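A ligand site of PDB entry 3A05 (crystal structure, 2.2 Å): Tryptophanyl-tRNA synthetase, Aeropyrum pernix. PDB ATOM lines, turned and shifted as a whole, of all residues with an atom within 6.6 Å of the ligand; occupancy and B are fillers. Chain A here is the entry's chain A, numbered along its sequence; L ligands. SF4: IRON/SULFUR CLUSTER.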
ATOM      1  N   LEU A 283      -4.573  24.476 -28.888  1.00  0.00           N
ATOM      2  CA  LEU A 283      -3.265  23.963 -28.486  1.00  0.00           C
ATOM      3  C   LEU A 283      -2.486  24.966 -27.665  1.00  0.00           C
ATOM      4  O   LEU A 283      -2.502  26.183 -27.932  1.00  0.00           O
ATOM      5  CB  LEU A 283      -2.449  23.447 -29.695  1.00  0.00           C
ATOM      6  CG  LEU A 283      -3.213  22.459 -30.617  1.00  0.00           C
ATOM      7  CD1 LEU A 283      -2.288  21.751 -31.615  1.00  0.00           C
ATOM      8  CD2 LEU A 283      -4.081  21.398 -29.871  1.00  0.00           C
ATOM      9  N   THR A 284      -1.795  24.451 -26.642  1.00  0.00           N
ATOM     10  CA  THR A 284      -1.062  25.297 -25.708  1.00  0.00           C
ATOM     11  C   THR A 284       0.401  24.916 -25.699  1.00  0.00           C
ATOM     12  O   THR A 284       0.807  23.981 -26.358  1.00  0.00           O
ATOM     13  CB  THR A 284      -1.620  25.109 -24.254  1.00  0.00           C
ATOM     14  OG1 THR A 284      -1.330  23.772 -23.816  1.00  0.00           O
ATOM     15  CG2 THR A 284      -3.137  25.343 -24.241  1.00  0.00           C
ATOM     16  N   GLY A 285       1.200  25.654 -24.965  1.00  0.00           N
ATOM     17  CA  GLY A 285       2.544  25.210 -24.657  1.00  0.00           C
ATOM     18  C   GLY A 285       2.597  24.599 -23.258  1.00  0.00           C
ATOM     19  O   GLY A 285       3.615  24.664 -22.602  1.00  0.00           O
ATOM     20  N   GLY A 286       1.475  24.037 -22.803  1.00  0.00           N
ATOM     21  CA  GLY A 286       1.372  23.491 -21.457  1.00  0.00           C
ATOM     22  C   GLY A 286       1.869  22.041 -21.389  1.00  0.00           C
ATOM     23  O   GLY A 286       2.301  21.475 -22.398  1.00  0.00           O
ATOM     24  N   ARG A 287       1.776  21.451 -20.198  1.00  0.00           N
ATOM     25  CA  ARG A 287       2.468  20.195 -19.904  1.00  0.00           C
ATOM     26  C   ARG A 287       1.523  19.016 -19.689  1.00  0.00           C
ATOM     27  O   ARG A 287       0.269  19.161 -19.759  1.00  0.00           O
ATOM     28  CB  ARG A 287       3.382  20.347 -18.686  1.00  0.00           C
ATOM     29  CG  ARG A 287       4.454  21.426 -18.780  1.00  0.00           C
ATOM     30  CD  ARG A 287       5.524  21.158 -19.827  1.00  0.00           C
ATOM     31  NE  ARG A 287       6.554  22.218 -19.759  1.00  0.00           N
ATOM     32  CZ  ARG A 287       7.741  22.153 -20.369  1.00  0.00           C
ATOM     33  NH1 ARG A 287       8.053  21.078 -21.093  1.00  0.00           N
ATOM     34  NH2 ARG A 287       8.609  23.159 -20.275  1.00  0.00           N
ATOM     35  N   GLN A 293       3.690  21.147 -14.909  1.00  0.00           N
ATOM     36  CA  GLN A 293       3.539  22.574 -15.233  1.00  0.00           C
ATOM     37  C   GLN A 293       4.083  23.463 -14.121  1.00  0.00           C
ATOM     38  O   GLN A 293       4.876  24.350 -14.372  1.00  0.00           O
ATOM     39  CB  GLN A 293       2.055  22.903 -15.499  1.00  0.00           C
ATOM     40  CG  GLN A 293       1.718  24.407 -15.529  1.00  0.00           C
ATOM     41  CD  GLN A 293       1.759  25.015 -16.927  1.00  0.00           C
ATOM     42  OE1 GLN A 293       1.338  24.377 -17.886  1.00  0.00           O
ATOM     43  NE2 GLN A 293       2.237  26.259 -17.025  1.00  0.00           N
ATOM     44  N   GLY A 297       7.032  25.124 -15.939  1.00  0.00           N
ATOM     45  CA  GLY A 297       6.304  26.237 -16.556  1.00  0.00           C
ATOM     46  C   GLY A 297       5.751  25.840 -17.921  1.00  0.00           C
ATOM     47  O   GLY A 297       5.950  24.701 -18.383  1.00  0.00           O
ATOM     48  N   GLY A 298       5.048  26.760 -18.566  1.00  0.00           N
ATOM     49  CA  GLY A 298       4.571  26.472 -19.922  1.00  0.00           C
ATOM     50  C   GLY A 298       5.490  27.128 -20.931  1.00  0.00           C
ATOM     51  O   GLY A 298       6.412  27.863 -20.550  1.00  0.00           O
ATOM     52  N   VAL A 299       5.220  26.876 -22.221  1.00  0.00           N
ATOM     53  CA  VAL A 299       5.965  27.476 -23.330  1.00  0.00           C
ATOM     54  C   VAL A 299       5.045  28.413 -24.187  1.00  0.00           C
ATOM     55  O   VAL A 299       4.382  27.956 -25.140  1.00  0.00           O
ATOM     56  CB  VAL A 299       6.663  26.366 -24.188  1.00  0.00           C
ATOM     57  CG1 VAL A 299       7.511  26.971 -25.311  1.00  0.00           C
ATOM     58  CG2 VAL A 299       7.527  25.456 -23.294  1.00  0.00           C
ATOM     59  N   PRO A 300       4.971  29.703 -23.821  1.00  0.00           N
ATOM     60  CA  PRO A 300       4.116  30.692 -24.527  1.00  0.00           C
ATOM     61  C   PRO A 300       4.437  30.916 -25.996  1.00  0.00           C
ATOM     62  O   PRO A 300       3.519  31.129 -26.789  1.00  0.00           O
ATOM     63  CB  PRO A 300       4.347  32.003 -23.752  1.00  0.00           C
ATOM     64  CG  PRO A 300       4.641  31.555 -22.356  1.00  0.00           C
ATOM     65  CD  PRO A 300       5.450  30.231 -22.525  1.00  0.00           C
ATOM     66  N   CYS A 303       2.319  28.658 -27.909  1.00  0.00           N
ATOM     67  CA  CYS A 303       0.974  28.488 -27.397  1.00  0.00           C
ATOM     68  C   CYS A 303       0.003  29.403 -28.126  1.00  0.00           C
ATOM     69  O   CYS A 303       0.151  30.642 -28.122  1.00  0.00           O
ATOM     70  CB  CYS A 303       0.948  28.863 -25.917  1.00  0.00           C
ATOM     71  SG  CYS A 303      -0.741  28.850 -25.343  1.00  0.00           S
ATOM     72  N   SER A 304      -1.054  28.800 -28.639  1.00  0.00           N
ATOM     73  CA  SER A 304      -2.023  29.553 -29.456  1.00  0.00           C
ATOM     74  C   SER A 304      -2.976  30.384 -28.569  1.00  0.00           C
ATOM     75  O   SER A 304      -3.663  31.315 -29.051  1.00  0.00           O
ATOM     76  CB  SER A 304      -2.793  28.584 -30.369  1.00  0.00           C
ATOM     77  OG  SER A 304      -3.872  27.990 -29.656  1.00  0.00           O
ATOM     78  N   VAL A 305      -3.020  30.067 -27.257  1.00  0.00           N
ATOM     79  CA  VAL A 305      -3.843  30.907 -26.352  1.00  0.00           C
ATOM     80  C   VAL A 305      -3.076  32.189 -26.066  1.00  0.00           C
ATOM     81  O   VAL A 305      -3.614  33.289 -26.153  1.00  0.00           O
ATOM     82  CB  VAL A 305      -4.167  30.198 -24.977  1.00  0.00           C
ATOM     83  CG1 VAL A 305      -4.942  31.156 -24.102  1.00  0.00           C
ATOM     84  CG2 VAL A 305      -4.955  28.825 -25.186  1.00  0.00           C
ATOM     85  N   TYR A 306      -1.806  32.037 -25.712  1.00  0.00           N
ATOM     86  CA  TYR A 306      -0.925  33.171 -25.557  1.00  0.00           C
ATOM     87  C   TYR A 306      -0.905  34.072 -26.809  1.00  0.00           C
ATOM     88  O   TYR A 306      -0.852  35.297 -26.699  1.00  0.00           O
ATOM     89  CB  TYR A 306       0.504  32.749 -25.209  1.00  0.00           C
ATOM     90  CG  TYR A 306       1.397  33.951 -25.016  1.00  0.00           C
ATOM     91  CD1 TYR A 306       1.177  34.852 -23.948  1.00  0.00           C
ATOM     92  CD2 TYR A 306       2.423  34.256 -25.942  1.00  0.00           C
ATOM     93  CE1 TYR A 306       1.971  35.963 -23.753  1.00  0.00           C
ATOM     94  CE2 TYR A 306       3.244  35.408 -25.785  1.00  0.00           C
ATOM     95  CZ  TYR A 306       3.013  36.257 -24.690  1.00  0.00           C
ATOM     96  OH  TYR A 306       3.801  37.388 -24.485  1.00  0.00           O
ATOM     97  N   ASP A 309      -3.945  36.147 -26.883  1.00  0.00           N
ATOM     98  CA  ASP A 309      -3.771  37.274 -25.951  1.00  0.00           C
ATOM     99  C   ASP A 309      -2.917  38.392 -26.564  1.00  0.00           C
ATOM    100  O   ASP A 309      -3.260  39.554 -26.468  1.00  0.00           O
ATOM    101  CB  ASP A 309      -3.110  36.790 -24.622  1.00  0.00           C
ATOM    102  CG  ASP A 309      -4.070  35.990 -23.715  1.00  0.00           C
ATOM    103  OD1 ASP A 309      -5.313  36.144 -23.786  1.00  0.00           O
ATOM    104  OD2 ASP A 309      -3.573  35.191 -22.907  1.00  0.00           O
ATOM    105  N   ILE A 323       0.895  37.492 -18.128  1.00  0.00           N
ATOM    106  CA  ILE A 323       0.554  36.127 -18.527  1.00  0.00           C
ATOM    107  C   ILE A 323       1.817  35.363 -18.945  1.00  0.00           C
ATOM    108  O   ILE A 323       1.984  34.202 -18.617  1.00  0.00           O
ATOM    109  CB  ILE A 323      -0.475  36.057 -19.697  1.00  0.00           C
ATOM    110  CG1 ILE A 323      -1.854  36.602 -19.273  1.00  0.00           C
ATOM    111  CG2 ILE A 323      -0.517  34.622 -20.290  1.00  0.00           C
ATOM    112  CD1 ILE A 323      -2.605  35.722 -18.277  1.00  0.00           C
ATOM    113  N   TYR A 324       2.669  36.019 -19.716  1.00  0.00           N
ATOM    114  CA  TYR A 324       3.919  35.391 -20.176  1.00  0.00           C
ATOM    115  C   TYR A 324       4.781  34.909 -19.003  1.00  0.00           C
ATOM    116  O   TYR A 324       5.298  33.779 -19.001  1.00  0.00           O
ATOM    117  CB  TYR A 324       4.709  36.392 -21.007  1.00  0.00           C
ATOM    118  CG  TYR A 324       6.029  35.876 -21.514  1.00  0.00           C
ATOM    119  CD1 TYR A 324       6.067  35.006 -22.619  1.00  0.00           C
ATOM    120  CD2 TYR A 324       7.243  36.269 -20.919  1.00  0.00           C
ATOM    121  CE1 TYR A 324       7.294  34.507 -23.120  1.00  0.00           C
ATOM    122  CE2 TYR A 324       8.486  35.783 -21.413  1.00  0.00           C
ATOM    123  CZ  TYR A 324       8.492  34.898 -22.508  1.00  0.00           C
ATOM    124  OH  TYR A 324       9.671  34.400 -23.009  1.00  0.00           O
ATOM    125  N   SER A 326       4.037  34.549 -15.581  1.00  0.00           N
ATOM    126  CA  SER A 326       3.391  33.524 -14.771  1.00  0.00           C
ATOM    127  C   SER A 326       3.514  32.149 -15.412  1.00  0.00           C
ATOM    128  O   SER A 326       4.078  31.205 -14.814  1.00  0.00           O
ATOM    129  CB  SER A 326       1.937  33.894 -14.503  1.00  0.00           C
ATOM    130  OG  SER A 326       1.853  35.216 -13.977  1.00  0.00           O
ATOM    131  N   CYS A 327       3.027  32.039 -16.651  1.00  0.00           N
ATOM    132  CA  CYS A 327       3.155  30.802 -17.415  1.00  0.00           C
ATOM    133  C   CYS A 327       4.556  30.185 -17.273  1.00  0.00           C
ATOM    134  O   CYS A 327       4.690  29.003 -16.885  1.00  0.00           O
ATOM    135  CB  CYS A 327       2.816  31.023 -18.887  1.00  0.00           C
ATOM    136  SG  CYS A 327       3.030  29.515 -19.862  1.00  0.00           S
ATOM    137  N   ARG A 328       5.579  30.967 -17.583  1.00  0.00           N
ATOM    138  CA  ARG A 328       6.946  30.493 -17.465  1.00  0.00           C
ATOM    139  C   ARG A 328       7.381  30.183 -16.004  1.00  0.00           C
ATOM    140  O   ARG A 328       7.982  29.129 -15.745  1.00  0.00           O
ATOM    141  CB  ARG A 328       7.914  31.499 -18.093  1.00  0.00           C
ATOM    142  CG  ARG A 328       7.879  31.449 -19.591  1.00  0.00           C
ATOM    143  CD  ARG A 328       8.965  32.269 -20.157  1.00  0.00           C
ATOM    144  NE  ARG A 328      10.130  31.467 -20.500  1.00  0.00           N
ATOM    145  CZ  ARG A 328      11.371  31.959 -20.568  1.00  0.00           C
ATOM    146  NH1 ARG A 328      11.599  33.245 -20.300  1.00  0.00           N
ATOM    147  NH2 ARG A 328      12.384  31.154 -20.910  1.00  0.00           N
ATOM    148  N   ILE A 332       0.836  29.471 -13.260  1.00  0.00           N
ATOM    149  CA  ILE A 332      -0.466  29.352 -13.923  1.00  0.00           C
ATOM    150  C   ILE A 332      -0.655  28.102 -14.794  1.00  0.00           C
ATOM    151  O   ILE A 332       0.237  27.667 -15.495  1.00  0.00           O
ATOM    152  CB  ILE A 332      -0.811  30.690 -14.724  1.00  0.00           C
ATOM    153  CG1 ILE A 332      -2.303  30.776 -15.108  1.00  0.00           C
ATOM    154  CG2 ILE A 332       0.107  30.890 -15.927  1.00  0.00           C
ATOM    155  CD1 ILE A 332      -2.612  32.096 -15.780  1.00  0.00           C
ATOM    156  N   LEU A 333      -1.850  27.559 -14.742  1.00  0.00           N
ATOM    157  CA  LEU A 333      -2.176  26.385 -15.476  1.00  0.00           C
ATOM    158  C   LEU A 333      -3.040  26.790 -16.659  1.00  0.00           C
ATOM    159  O   LEU A 333      -3.765  27.813 -16.603  1.00  0.00           O
ATOM    160  CB  LEU A 333      -2.929  25.416 -14.577  1.00  0.00           C
ATOM    161  CG  LEU A 333      -2.314  24.957 -13.233  1.00  0.00           C
ATOM    162  CD1 LEU A 333      -3.126  23.803 -12.670  1.00  0.00           C
ATOM    163  CD2 LEU A 333      -0.816  24.566 -13.315  1.00  0.00           C
ATOM    164  N   CYS A 334      -3.007  25.958 -17.705  1.00  0.00           N
ATOM    165  CA  CYS A 334      -3.661  26.247 -18.980  1.00  0.00           C
ATOM    166  C   CYS A 334      -5.130  26.454 -18.797  1.00  0.00           C
ATOM    167  O   CYS A 334      -5.697  27.362 -19.432  1.00  0.00           O
ATOM    168  CB  CYS A 334      -3.396  25.146 -20.014  1.00  0.00           C
ATOM    169  SG  CYS A 334      -1.640  25.060 -20.438  1.00  0.00           S
ATOM    170  N   GLY A 335      -5.744  25.636 -17.930  1.00  0.00           N
ATOM    171  CA  GLY A 335      -7.179  25.748 -17.706  1.00  0.00           C
ATOM    172  C   GLY A 335      -7.559  27.146 -17.271  1.00  0.00           C
ATOM    173  O   GLY A 335      -8.573  27.717 -17.726  1.00  0.00           O
ATOM    174  N   CYS A 337      -5.640  29.969 -17.512  1.00  0.00           N
ATOM    175  CA  CYS A 337      -5.178  30.803 -18.592  1.00  0.00           C
ATOM    176  C   CYS A 337      -6.222  30.942 -19.706  1.00  0.00           C
ATOM    177  O   CYS A 337      -6.549  32.067 -20.114  1.00  0.00           O
ATOM    178  CB  CYS A 337      -3.878  30.216 -19.142  1.00  0.00           C
ATOM    179  SG  CYS A 337      -2.871  31.513 -19.975  1.00  0.00           S
ATOM    180  N   LYS A 338      -6.780  29.792 -20.115  1.00  0.00           N
ATOM    181  CA  LYS A 338      -7.845  29.689 -21.088  1.00  0.00           C
ATOM    182  C   LYS A 338      -9.083  30.404 -20.633  1.00  0.00           C
ATOM    183  O   LYS A 338      -9.738  31.093 -21.445  1.00  0.00           O
ATOM    184  CB  LYS A 338      -8.187  28.221 -21.406  1.00  0.00           C
ATOM    185  CG  LYS A 338      -7.215  27.597 -22.456  1.00  0.00           C
ATOM    186  CD  LYS A 338      -7.502  26.100 -22.733  1.00  0.00           C
ATOM    187  CE  LYS A 338      -6.493  25.555 -23.777  1.00  0.00           C
ATOM    188  NZ  LYS A 338      -6.788  24.104 -24.136  1.00  0.00           N
HETATM  189 FE1  SF4 L   1       1.075  29.007 -20.633  1.00  0.00          FE
HETATM  190 FE2  SF4 L   1      -1.486  30.036 -20.859  1.00  0.00          FE
HETATM  191 FE3  SF4 L   1      -0.337  28.994 -23.019  1.00  0.00          FE
HETATM  192 FE4  SF4 L   1      -0.980  27.270 -20.828  1.00  0.00          FE
HETATM  193  S1  SF4 L   1      -2.438  28.438 -22.171  1.00  0.00           S
HETATM  194  S2  SF4 L   1       0.941  27.239 -22.087  1.00  0.00           S
HETATM  195  S3  SF4 L   1      -0.608  28.773 -19.105  1.00  0.00           S
HETATM  196  S4  SF4 L   1       0.380  30.833 -21.977  1.00  0.00           S
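The backbone NH of Gly 286 sits close to a sulfur (S2) of the ligand, 3.3 Å away.
A sulfur (S2) of the ligand lies close to the backbone NH (N) of Gly 285.
An iron atom (FE1) of the ligand is bound by the side-chain sulfur (SG) of Cys 327 (2.2 Å).
The side-chain sulfur (SG) of Cys 334 is bound to an iron atom (FE4) of the ligand (2.3 Å).
The side-chain sulfur (SG) of Cys 303 is bound to an iron atom (FE3) of the ligand (2.4 Å).
An iron atom (FE2) of the ligand is bound by the side-chain sulfur (SG) of Cys 337, 2.2 Å away.
N of Gly 285 lies close to SG of Cys 303, 3.8 Å away.
OG1 of Thr 284 lies within hydrogen-bond range of N of Gly 286.
The backbone carbonyl oxygen (O) of Ile 332 is in hydrogen-bond range of the side-chain amide nitrogen (NE2) of Gln 293 (2.9 Å).
The backbone NH (N) of Gly 298 is in hydrogen-bond range of the backbone carbonyl oxygen (O) of Cys 327 (2.8 Å).
N of Val 305 lies close to SG of Cys 303.
The backbone carbonyl oxygen of Gly 285 lies within hydrogen-bond range of the backbone NH of Val 299 (2.8 Å).
The side-chain hydroxyl of Thr 284 lies close to the side-chain sulfur of Cys 334, at 3.6 Å.
SG of Cys 303 sits close to N of Tyr 306.
Thr 284 touches the ligand.
Val 305 touches the ligand.
Tyr 306 touches the ligand (CB to S4, 3.8 Å).
Ile 332 touches the ligand (O to S3, 3.9 Å).
C of Leu 333 touches S3 of the ligand, 3.98 Å away.
The nearest printed residue that does not touch the ligand is Ile 323 (4.2 Å).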
